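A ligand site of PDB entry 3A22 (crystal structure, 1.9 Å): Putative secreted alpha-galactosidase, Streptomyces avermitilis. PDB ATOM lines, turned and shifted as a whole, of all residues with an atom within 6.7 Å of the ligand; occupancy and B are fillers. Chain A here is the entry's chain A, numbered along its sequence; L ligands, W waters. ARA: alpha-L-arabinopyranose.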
ATOM      1  N   TRP A  19      -3.235  22.705 -23.957  1.00  0.00           N
ATOM      2  CA  TRP A  19      -3.669  22.609 -22.557  1.00  0.00           C
ATOM      3  C   TRP A  19      -3.121  23.682 -21.611  1.00  0.00           C
ATOM      4  O   TRP A  19      -3.893  24.358 -20.965  1.00  0.00           O
ATOM      5  CB  TRP A  19      -3.422  21.208 -21.957  1.00  0.00           C
ATOM      6  CG  TRP A  19      -3.990  21.131 -20.560  1.00  0.00           C
ATOM      7  CD1 TRP A  19      -3.292  21.119 -19.382  1.00  0.00           C
ATOM      8  CD2 TRP A  19      -5.382  21.156 -20.204  1.00  0.00           C
ATOM      9  NE1 TRP A  19      -4.163  21.109 -18.317  1.00  0.00           N
ATOM     10  CE2 TRP A  19      -5.444  21.143 -18.798  1.00  0.00           C
ATOM     11  CE3 TRP A  19      -6.572  21.184 -20.942  1.00  0.00           C
ATOM     12  CZ2 TRP A  19      -6.673  21.135 -18.105  1.00  0.00           C
ATOM     13  CZ3 TRP A  19      -7.779  21.179 -20.261  1.00  0.00           C
ATOM     14  CH2 TRP A  19      -7.827  21.154 -18.846  1.00  0.00           C
ATOM     15  N   ASN A  20      -1.796  23.807 -21.526  1.00  0.00           N
ATOM     16  CA  ASN A  20      -1.172  24.622 -20.473  1.00  0.00           C
ATOM     17  C   ASN A  20      -1.654  26.087 -20.462  1.00  0.00           C
ATOM     18  O   ASN A  20      -1.859  26.673 -19.399  1.00  0.00           O
ATOM     19  CB  ASN A  20       0.375  24.555 -20.566  1.00  0.00           C
ATOM     20  CG  ASN A  20       0.959  23.213 -20.057  1.00  0.00           C
ATOM     21  OD1 ASN A  20       0.233  22.299 -19.623  1.00  0.00           O
ATOM     22  ND2 ASN A  20       2.291  23.098 -20.094  1.00  0.00           N
ATOM     23  N   ASP A  54      -5.929  19.564 -27.343  1.00  0.00           N
ATOM     24  CA  ASP A  54      -6.081  18.827 -26.102  1.00  0.00           C
ATOM     25  C   ASP A  54      -7.557  18.879 -25.677  1.00  0.00           C
ATOM     26  O   ASP A  54      -8.432  19.100 -26.507  1.00  0.00           O
ATOM     27  CB  ASP A  54      -5.134  19.432 -25.059  1.00  0.00           C
ATOM     28  CG  ASP A  54      -4.740  18.443 -23.948  1.00  0.00           C
ATOM     29  OD1 ASP A  54      -5.589  18.189 -23.065  1.00  0.00           O
ATOM     30  OD2 ASP A  54      -3.593  17.960 -23.927  1.00  0.00           O
ATOM     31  N   GLU A  55      -7.841  18.685 -24.391  1.00  0.00           N
ATOM     32  CA  GLU A  55      -9.208  18.666 -23.863  1.00  0.00           C
ATOM     33  C   GLU A  55      -9.972  19.931 -24.218  1.00  0.00           C
ATOM     34  O   GLU A  55      -9.425  21.034 -24.123  1.00  0.00           O
ATOM     35  CB  GLU A  55      -9.174  18.522 -22.337  1.00  0.00           C
ATOM     36  CG  GLU A  55     -10.532  18.561 -21.668  1.00  0.00           C
ATOM     37  CD  GLU A  55     -10.451  18.755 -20.161  1.00  0.00           C
ATOM     38  OE1 GLU A  55      -9.592  18.125 -19.524  1.00  0.00           O
ATOM     39  OE2 GLU A  55     -11.276  19.521 -19.622  1.00  0.00           O
ATOM     40  N   TYR A  96      -7.349  14.312 -28.871  1.00  0.00           N
ATOM     41  CA  TYR A  96      -7.386  13.988 -27.441  1.00  0.00           C
ATOM     42  C   TYR A  96      -8.704  13.307 -27.072  1.00  0.00           C
ATOM     43  O   TYR A  96      -9.787  13.791 -27.444  1.00  0.00           O
ATOM     44  CB  TYR A  96      -7.239  15.292 -26.640  1.00  0.00           C
ATOM     45  CG  TYR A  96      -7.470  15.156 -25.143  1.00  0.00           C
ATOM     46  CD1 TYR A  96      -8.748  15.284 -24.600  1.00  0.00           C
ATOM     47  CD2 TYR A  96      -6.402  14.908 -24.279  1.00  0.00           C
ATOM     48  CE1 TYR A  96      -8.968  15.159 -23.234  1.00  0.00           C
ATOM     49  CE2 TYR A  96      -6.613  14.781 -22.884  1.00  0.00           C
ATOM     50  CZ  TYR A  96      -7.892  14.912 -22.387  1.00  0.00           C
ATOM     51  OH  TYR A  96      -8.115  14.792 -21.033  1.00  0.00           O
ATOM     52  N   ASP A  98     -10.338   9.952 -23.974  1.00  0.00           N
ATOM     53  CA  ASP A  98     -10.135   9.230 -22.713  1.00  0.00           C
ATOM     54  C   ASP A  98     -10.277   7.746 -22.957  1.00  0.00           C
ATOM     55  O   ASP A  98     -11.024   7.336 -23.846  1.00  0.00           O
ATOM     56  CB  ASP A  98     -11.195   9.615 -21.679  1.00  0.00           C
ATOM     57  CG  ASP A  98     -10.695   9.452 -20.267  1.00  0.00           C
ATOM     58  OD1 ASP A  98     -10.089  10.418 -19.734  1.00  0.00           O
ATOM     59  OD2 ASP A  98     -10.887   8.351 -19.696  1.00  0.00           O
ATOM     60  N   CYS A 104     -11.843  13.725 -18.996  1.00  0.00           N
ATOM     61  CA  CYS A 104     -11.460  14.688 -17.969  1.00  0.00           C
ATOM     62  C   CYS A 104     -12.328  15.949 -18.006  1.00  0.00           C
ATOM     63  O   CYS A 104     -12.521  16.585 -16.971  1.00  0.00           O
ATOM     64  CB  CYS A 104      -9.959  15.020 -18.026  1.00  0.00           C
ATOM     65  SG  CYS A 104      -8.907  13.574 -17.779  1.00  0.00           S
ATOM     66  N   GLY A 105     -12.867  16.278 -19.188  1.00  0.00           N
ATOM     67  CA  GLY A 105     -13.828  17.394 -19.355  1.00  0.00           C
ATOM     68  C   GLY A 105     -15.152  17.125 -18.647  1.00  0.00           C
ATOM     69  O   GLY A 105     -15.981  18.033 -18.438  1.00  0.00           O
ATOM     70  N   TYR A 108     -13.292  16.534 -14.334  1.00  0.00           N
ATOM     71  CA  TYR A 108     -12.589  17.711 -13.815  1.00  0.00           C
ATOM     72  C   TYR A 108     -12.781  18.904 -14.761  1.00  0.00           C
ATOM     73  O   TYR A 108     -11.838  19.360 -15.433  1.00  0.00           O
ATOM     74  CB  TYR A 108     -11.095  17.407 -13.630  1.00  0.00           C
ATOM     75  CG  TYR A 108     -10.775  16.210 -12.752  1.00  0.00           C
ATOM     76  CD1 TYR A 108     -10.768  16.339 -11.353  1.00  0.00           C
ATOM     77  CD2 TYR A 108     -10.474  14.974 -13.302  1.00  0.00           C
ATOM     78  CE1 TYR A 108     -10.457  15.250 -10.535  1.00  0.00           C
ATOM     79  CE2 TYR A 108     -10.156  13.871 -12.492  1.00  0.00           C
ATOM     80  CZ  TYR A 108     -10.154  14.019 -11.107  1.00  0.00           C
ATOM     81  OH  TYR A 108      -9.828  12.947 -10.293  1.00  0.00           O
ATOM     82  N   LYS A 140      -3.686  11.764 -27.937  1.00  0.00           N
ATOM     83  CA  LYS A 140      -3.358  11.685 -26.515  1.00  0.00           C
ATOM     84  C   LYS A 140      -4.550  11.034 -25.829  1.00  0.00           C
ATOM     85  O   LYS A 140      -5.694  11.514 -25.962  1.00  0.00           O
ATOM     86  CB  LYS A 140      -3.102  13.096 -25.950  1.00  0.00           C
ATOM     87  CG  LYS A 140      -2.795  13.181 -24.436  1.00  0.00           C
ATOM     88  CD  LYS A 140      -2.498  14.646 -24.076  1.00  0.00           C
ATOM     89  CE  LYS A 140      -2.504  14.868 -22.570  1.00  0.00           C
ATOM     90  NZ  LYS A 140      -2.244  16.297 -22.218  1.00  0.00           N
ATOM     91  N   ASP A 142      -6.214   9.997 -22.416  1.00  0.00           N
ATOM     92  CA  ASP A 142      -6.208  10.258 -20.982  1.00  0.00           C
ATOM     93  C   ASP A 142      -6.903   9.154 -20.158  1.00  0.00           C
ATOM     94  O   ASP A 142      -7.409   8.174 -20.718  1.00  0.00           O
ATOM     95  CB  ASP A 142      -6.858  11.630 -20.709  1.00  0.00           C
ATOM     96  CG  ASP A 142      -6.224  12.350 -19.527  1.00  0.00           C
ATOM     97  OD1 ASP A 142      -5.844  11.702 -18.523  1.00  0.00           O
ATOM     98  OD2 ASP A 142      -6.120  13.596 -19.600  1.00  0.00           O
ATOM     99  N   TRP A 143      -6.953   9.351 -18.835  1.00  0.00           N
ATOM    100  CA  TRP A 143      -7.263   8.262 -17.896  1.00  0.00           C
ATOM    101  C   TRP A 143      -8.377   8.600 -16.879  1.00  0.00           C
ATOM    102  O   TRP A 143      -8.614   7.833 -15.955  1.00  0.00           O
ATOM    103  CB  TRP A 143      -5.977   7.869 -17.165  1.00  0.00           C
ATOM    104  CG  TRP A 143      -6.053   6.623 -16.351  1.00  0.00           C
ATOM    105  CD1 TRP A 143      -5.801   6.501 -15.027  1.00  0.00           C
ATOM    106  CD2 TRP A 143      -6.362   5.303 -16.842  1.00  0.00           C
ATOM    107  NE1 TRP A 143      -5.963   5.187 -14.634  1.00  0.00           N
ATOM    108  CE2 TRP A 143      -6.319   4.432 -15.724  1.00  0.00           C
ATOM    109  CE3 TRP A 143      -6.697   4.782 -18.101  1.00  0.00           C
ATOM    110  CZ2 TRP A 143      -6.590   3.052 -15.832  1.00  0.00           C
ATOM    111  CZ3 TRP A 143      -6.969   3.403 -18.209  1.00  0.00           C
ATOM    112  CH2 TRP A 143      -6.923   2.561 -17.079  1.00  0.00           C
ATOM    113  N   CYS A 144      -9.028   9.746 -17.027  1.00  0.00           N
ATOM    114  CA  CYS A 144     -10.052  10.134 -16.030  1.00  0.00           C
ATOM    115  C   CYS A 144     -11.171   9.091 -15.909  1.00  0.00           C
ATOM    116  O   CYS A 144     -11.586   8.728 -14.795  1.00  0.00           O
ATOM    117  CB  CYS A 144     -10.616  11.536 -16.312  1.00  0.00           C
ATOM    118  SG  CYS A 144      -9.450  12.891 -15.953  1.00  0.00           S
ATOM    119  N   CYS A 180      -1.622   8.847 -21.510  1.00  0.00           N
ATOM    120  CA  CYS A 180      -1.698   9.881 -20.468  1.00  0.00           C
ATOM    121  C   CYS A 180      -2.436   9.346 -19.244  1.00  0.00           C
ATOM    122  O   CYS A 180      -3.665   9.509 -19.128  1.00  0.00           O
ATOM    123  CB  CYS A 180      -2.344  11.156 -21.032  1.00  0.00           C
ATOM    124  SG  CYS A 180      -2.467  12.491 -19.831  1.00  0.00           S
ATOM    125  N   ASN A 181      -1.699   8.642 -18.378  1.00  0.00           N
ATOM    126  CA  ASN A 181      -2.300   8.050 -17.183  1.00  0.00           C
ATOM    127  C   ASN A 181      -1.516   8.402 -15.912  1.00  0.00           C
ATOM    128  O   ASN A 181      -1.722   7.812 -14.846  1.00  0.00           O
ATOM    129  CB  ASN A 181      -2.623   6.540 -17.354  1.00  0.00           C
ATOM    130  CG  ASN A 181      -1.609   5.608 -16.692  1.00  0.00           C
ATOM    131  OD1 ASN A 181      -0.415   5.703 -16.915  1.00  0.00           O
ATOM    132  ND2 ASN A 181      -2.121   4.649 -15.906  1.00  0.00           N
ATOM    133  N   TRP A 182      -0.664   9.410 -16.040  1.00  0.00           N
ATOM    134  CA  TRP A 182      -0.150  10.177 -14.899  1.00  0.00           C
ATOM    135  C   TRP A 182       0.780   9.391 -13.976  1.00  0.00           C
ATOM    136  O   TRP A 182       0.952   9.759 -12.804  1.00  0.00           O
ATOM    137  CB  TRP A 182      -1.309  10.759 -14.041  1.00  0.00           C
ATOM    138  CG  TRP A 182      -2.617  11.069 -14.772  1.00  0.00           C
ATOM    139  CD1 TRP A 182      -2.767  11.741 -15.971  1.00  0.00           C
ATOM    140  CD2 TRP A 182      -3.935  10.726 -14.334  1.00  0.00           C
ATOM    141  NE1 TRP A 182      -4.109  11.808 -16.291  1.00  0.00           N
ATOM    142  CE2 TRP A 182      -4.843  11.202 -15.303  1.00  0.00           C
ATOM    143  CE3 TRP A 182      -4.434  10.023 -13.209  1.00  0.00           C
ATOM    144  CZ2 TRP A 182      -6.233  11.017 -15.197  1.00  0.00           C
ATOM    145  CZ3 TRP A 182      -5.823   9.847 -13.091  1.00  0.00           C
ATOM    146  CH2 TRP A 182      -6.705  10.362 -14.081  1.00  0.00           C
ATOM    147  N   ARG A 199       2.905   9.341 -20.029  1.00  0.00           N
ATOM    148  CA  ARG A 199       3.030  10.231 -18.902  1.00  0.00           C
ATOM    149  C   ARG A 199       3.478   9.505 -17.624  1.00  0.00           C
ATOM    150  O   ARG A 199       2.928   8.447 -17.289  1.00  0.00           O
ATOM    151  CB  ARG A 199       1.735  11.020 -18.671  1.00  0.00           C
ATOM    152  CG  ARG A 199       1.476  12.156 -19.699  1.00  0.00           C
ATOM    153  CD  ARG A 199       2.159  13.484 -19.314  1.00  0.00           C
ATOM    154  NE  ARG A 199       1.752  13.858 -17.965  1.00  0.00           N
ATOM    155  CZ  ARG A 199       0.594  14.447 -17.662  1.00  0.00           C
ATOM    156  NH1 ARG A 199      -0.272  14.779 -18.633  1.00  0.00           N
ATOM    157  NH2 ARG A 199       0.300  14.683 -16.389  1.00  0.00           N
ATOM    158  N   SER A 201       3.812  11.082 -14.432  1.00  0.00           N
ATOM    159  CA  SER A 201       3.354  11.788 -13.209  1.00  0.00           C
ATOM    160  C   SER A 201       2.109  12.621 -13.473  1.00  0.00           C
ATOM    161  O   SER A 201       1.652  12.709 -14.613  1.00  0.00           O
ATOM    162  CB  SER A 201       4.447  12.735 -12.676  1.00  0.00           C
ATOM    163  OG  SER A 201       4.617  13.792 -13.600  1.00  0.00           O
ATOM    164  N   THR A 202       1.589  13.250 -12.421  1.00  0.00           N
ATOM    165  CA  THR A 202       0.462  14.152 -12.553  1.00  0.00           C
ATOM    166  C   THR A 202       0.945  15.449 -13.217  1.00  0.00           C
ATOM    167  O   THR A 202       2.138  15.586 -13.531  1.00  0.00           O
ATOM    168  CB  THR A 202      -0.207  14.435 -11.196  1.00  0.00           C
ATOM    169  OG1 THR A 202       0.795  14.875 -10.261  1.00  0.00           O
ATOM    170  CG2 THR A 202      -0.904  13.138 -10.669  1.00  0.00           C
ATOM    171  N   ASP A 203       0.020  16.380 -13.433  1.00  0.00           N
ATOM    172  CA  ASP A 203       0.243  17.538 -14.316  1.00  0.00           C
ATOM    173  C   ASP A 203       1.304  18.504 -13.823  1.00  0.00           C
ATOM    174  O   ASP A 203       1.335  18.877 -12.636  1.00  0.00           O
ATOM    175  CB  ASP A 203      -1.057  18.298 -14.553  1.00  0.00           C
ATOM    176  CG  ASP A 203      -2.170  17.427 -15.096  1.00  0.00           C
ATOM    177  OD1 ASP A 203      -1.955  16.205 -15.386  1.00  0.00           O
ATOM    178  OD2 ASP A 203      -3.288  17.963 -15.226  1.00  0.00           O
ATOM    179  N   TYR A 206      -1.448  23.278 -13.043  1.00  0.00           N
ATOM    180  CA  TYR A 206      -2.907  23.310 -12.961  1.00  0.00           C
ATOM    181  C   TYR A 206      -3.415  24.712 -13.270  1.00  0.00           C
ATOM    182  O   TYR A 206      -2.865  25.706 -12.799  1.00  0.00           O
ATOM    183  CB  TYR A 206      -3.402  22.781 -11.596  1.00  0.00           C
ATOM    184  CG  TYR A 206      -3.192  21.290 -11.515  1.00  0.00           C
ATOM    185  CD1 TYR A 206      -1.978  20.762 -11.096  1.00  0.00           C
ATOM    186  CD2 TYR A 206      -4.187  20.407 -11.939  1.00  0.00           C
ATOM    187  CE1 TYR A 206      -1.769  19.373 -11.072  1.00  0.00           C
ATOM    188  CE2 TYR A 206      -3.988  19.038 -11.920  1.00  0.00           C
ATOM    189  CZ  TYR A 206      -2.781  18.524 -11.493  1.00  0.00           C
ATOM    190  OH  TYR A 206      -2.597  17.149 -11.505  1.00  0.00           O
ATOM    191  N   ASP A 238       5.853  15.609 -19.176  1.00  0.00           N
ATOM    192  CA  ASP A 238       4.702  16.509 -19.446  1.00  0.00           C
ATOM    193  C   ASP A 238       5.058  17.703 -20.348  1.00  0.00           C
ATOM    194  O   ASP A 238       6.238  17.954 -20.657  1.00  0.00           O
ATOM    195  CB  ASP A 238       3.971  16.942 -18.144  1.00  0.00           C
ATOM    196  CG  ASP A 238       2.470  17.215 -18.333  1.00  0.00           C
ATOM    197  OD1 ASP A 238       1.931  17.159 -19.471  1.00  0.00           O
ATOM    198  OD2 ASP A 238       1.810  17.528 -17.311  1.00  0.00           O
ATOM    199  N   MET A 239       4.020  18.415 -20.763  1.00  0.00           N
ATOM    200  CA  MET A 239       4.112  19.570 -21.659  1.00  0.00           C
ATOM    201  C   MET A 239       4.939  20.692 -21.040  1.00  0.00           C
ATOM    202  O   MET A 239       4.891  20.924 -19.829  1.00  0.00           O
ATOM    203  CB  MET A 239       2.707  20.047 -22.022  1.00  0.00           C
ATOM    204  CG  MET A 239       1.914  19.009 -22.815  1.00  0.00           C
ATOM    205  SD  MET A 239       0.131  19.272 -22.870  1.00  0.00           S
ATOM    206  CE  MET A 239      -0.284  19.342 -21.118  1.00  0.00           C
HETATM  207  C1  ARA L   1      -5.383  15.923 -17.696  1.00  0.00           C
HETATM  208  C2  ARA L   1      -4.065  15.740 -18.444  1.00  0.00           C
HETATM  209  C3  ARA L   1      -3.562  17.100 -18.926  1.00  0.00           C
HETATM  210  C4  ARA L   1      -4.637  17.695 -19.849  1.00  0.00           C
HETATM  211  C5  ARA L   1      -5.972  17.766 -19.099  1.00  0.00           C
HETATM  212  O1  ARA L   1      -5.835  14.668 -17.185  1.00  0.00           O
HETATM  213  O2  ARA L   1      -3.132  15.059 -17.631  1.00  0.00           O
HETATM  214  O3  ARA L   1      -2.342  16.975 -19.636  1.00  0.00           O
HETATM  215  O4  ARA L   1      -4.756  16.802 -20.939  1.00  0.00           O
HETATM  216  O5  ARA L   1      -6.345  16.476 -18.581  1.00  0.00           O
HETATM  217  O   HOH W   1      -0.786  18.214 -17.924  1.00  0.00           O
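An oxygen (O2) of the ligand sits at hydrogen-bond distance from the side-chain sulfur (SG) of Cys 180 (3.4 Å).
SG of Cys 104 is in hydrogen-bond range of O1 of the ligand (3.3 Å).
O5 of the ligand sits at hydrogen-bond distance from OH of Tyr 96 (3.5 Å).
The side-chain carboxylate of Asp 203 lies within hydrogen-bond range of an oxygen (O2) of the ligand.
OD1 of Asp 54 sits at hydrogen-bond distance from O4 of the ligand (2.7 Å).
The side-chain carboxylate of Asp 142 lies within hydrogen-bond range of an oxygen (O1) of the ligand, 2.7 Å away.
An oxygen (O3) of the ligand sits at hydrogen-bond distance from the side-chain amino group of Lys 140 (2.7 Å).
NH1 of Arg 199 sits at hydrogen-bond distance from O2 of the ligand.
An oxygen (O1) of the ligand is in hydrogen-bond range of the indole nitrogen of Trp 182, 3.5 Å away.
OD1 of Asp 142 lies within hydrogen-bond range of NE1 of Trp 182 (2.8 Å).
The side-chain sulfur (SG) of Cys 104 sits close to the side-chain hydroxyl (OH) of Tyr 96, 3.6 Å away.
The side-chain sulfur (SG) of Cys 144 is disulfide-bonded to the side-chain sulfur (SG) of Cys 104 (2.0 Å).
The side-chain carboxylate (OD1) of Asp 203 is in salt-bridge range of the guanidinium group (NH2) of Arg 199 (2.9 Å).
The backbone carbonyl oxygen (O) of Cys 180 sits at hydrogen-bond distance from the backbone NH (N) of Trp 143 (3.3 Å).
OD1 of Asp 142 is in hydrogen-bond range of SG of Cys 180.
NH2 of Arg 199 sits at hydrogen-bond distance from O of Ser 201.
The side-chain carboxylate of Asp 54 lies within salt-bridge range of the side-chain amino group of Lys 140, 2.7 Å away.
Trp 19 touches the ligand (CE2 to C5, 3.4 Å).
Glu 55 touches the ligand (OE1 to C5, 3.7 Å).
Met 239 touches the ligand.
Hydrophobic or aromatic side chains that line the ligand: Trp 19, Tyr 96, Trp 182 and Met 239.
The nearest printed residue that does not touch the ligand is Cys 144 (4.2 Å).
Water W1 lies within hydrogen-bond range of O3 of the ligand (2.6 Å), OD2 of Asp 238 (2.8 Å) and OD1 of Asp 203 (3.4 Å).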
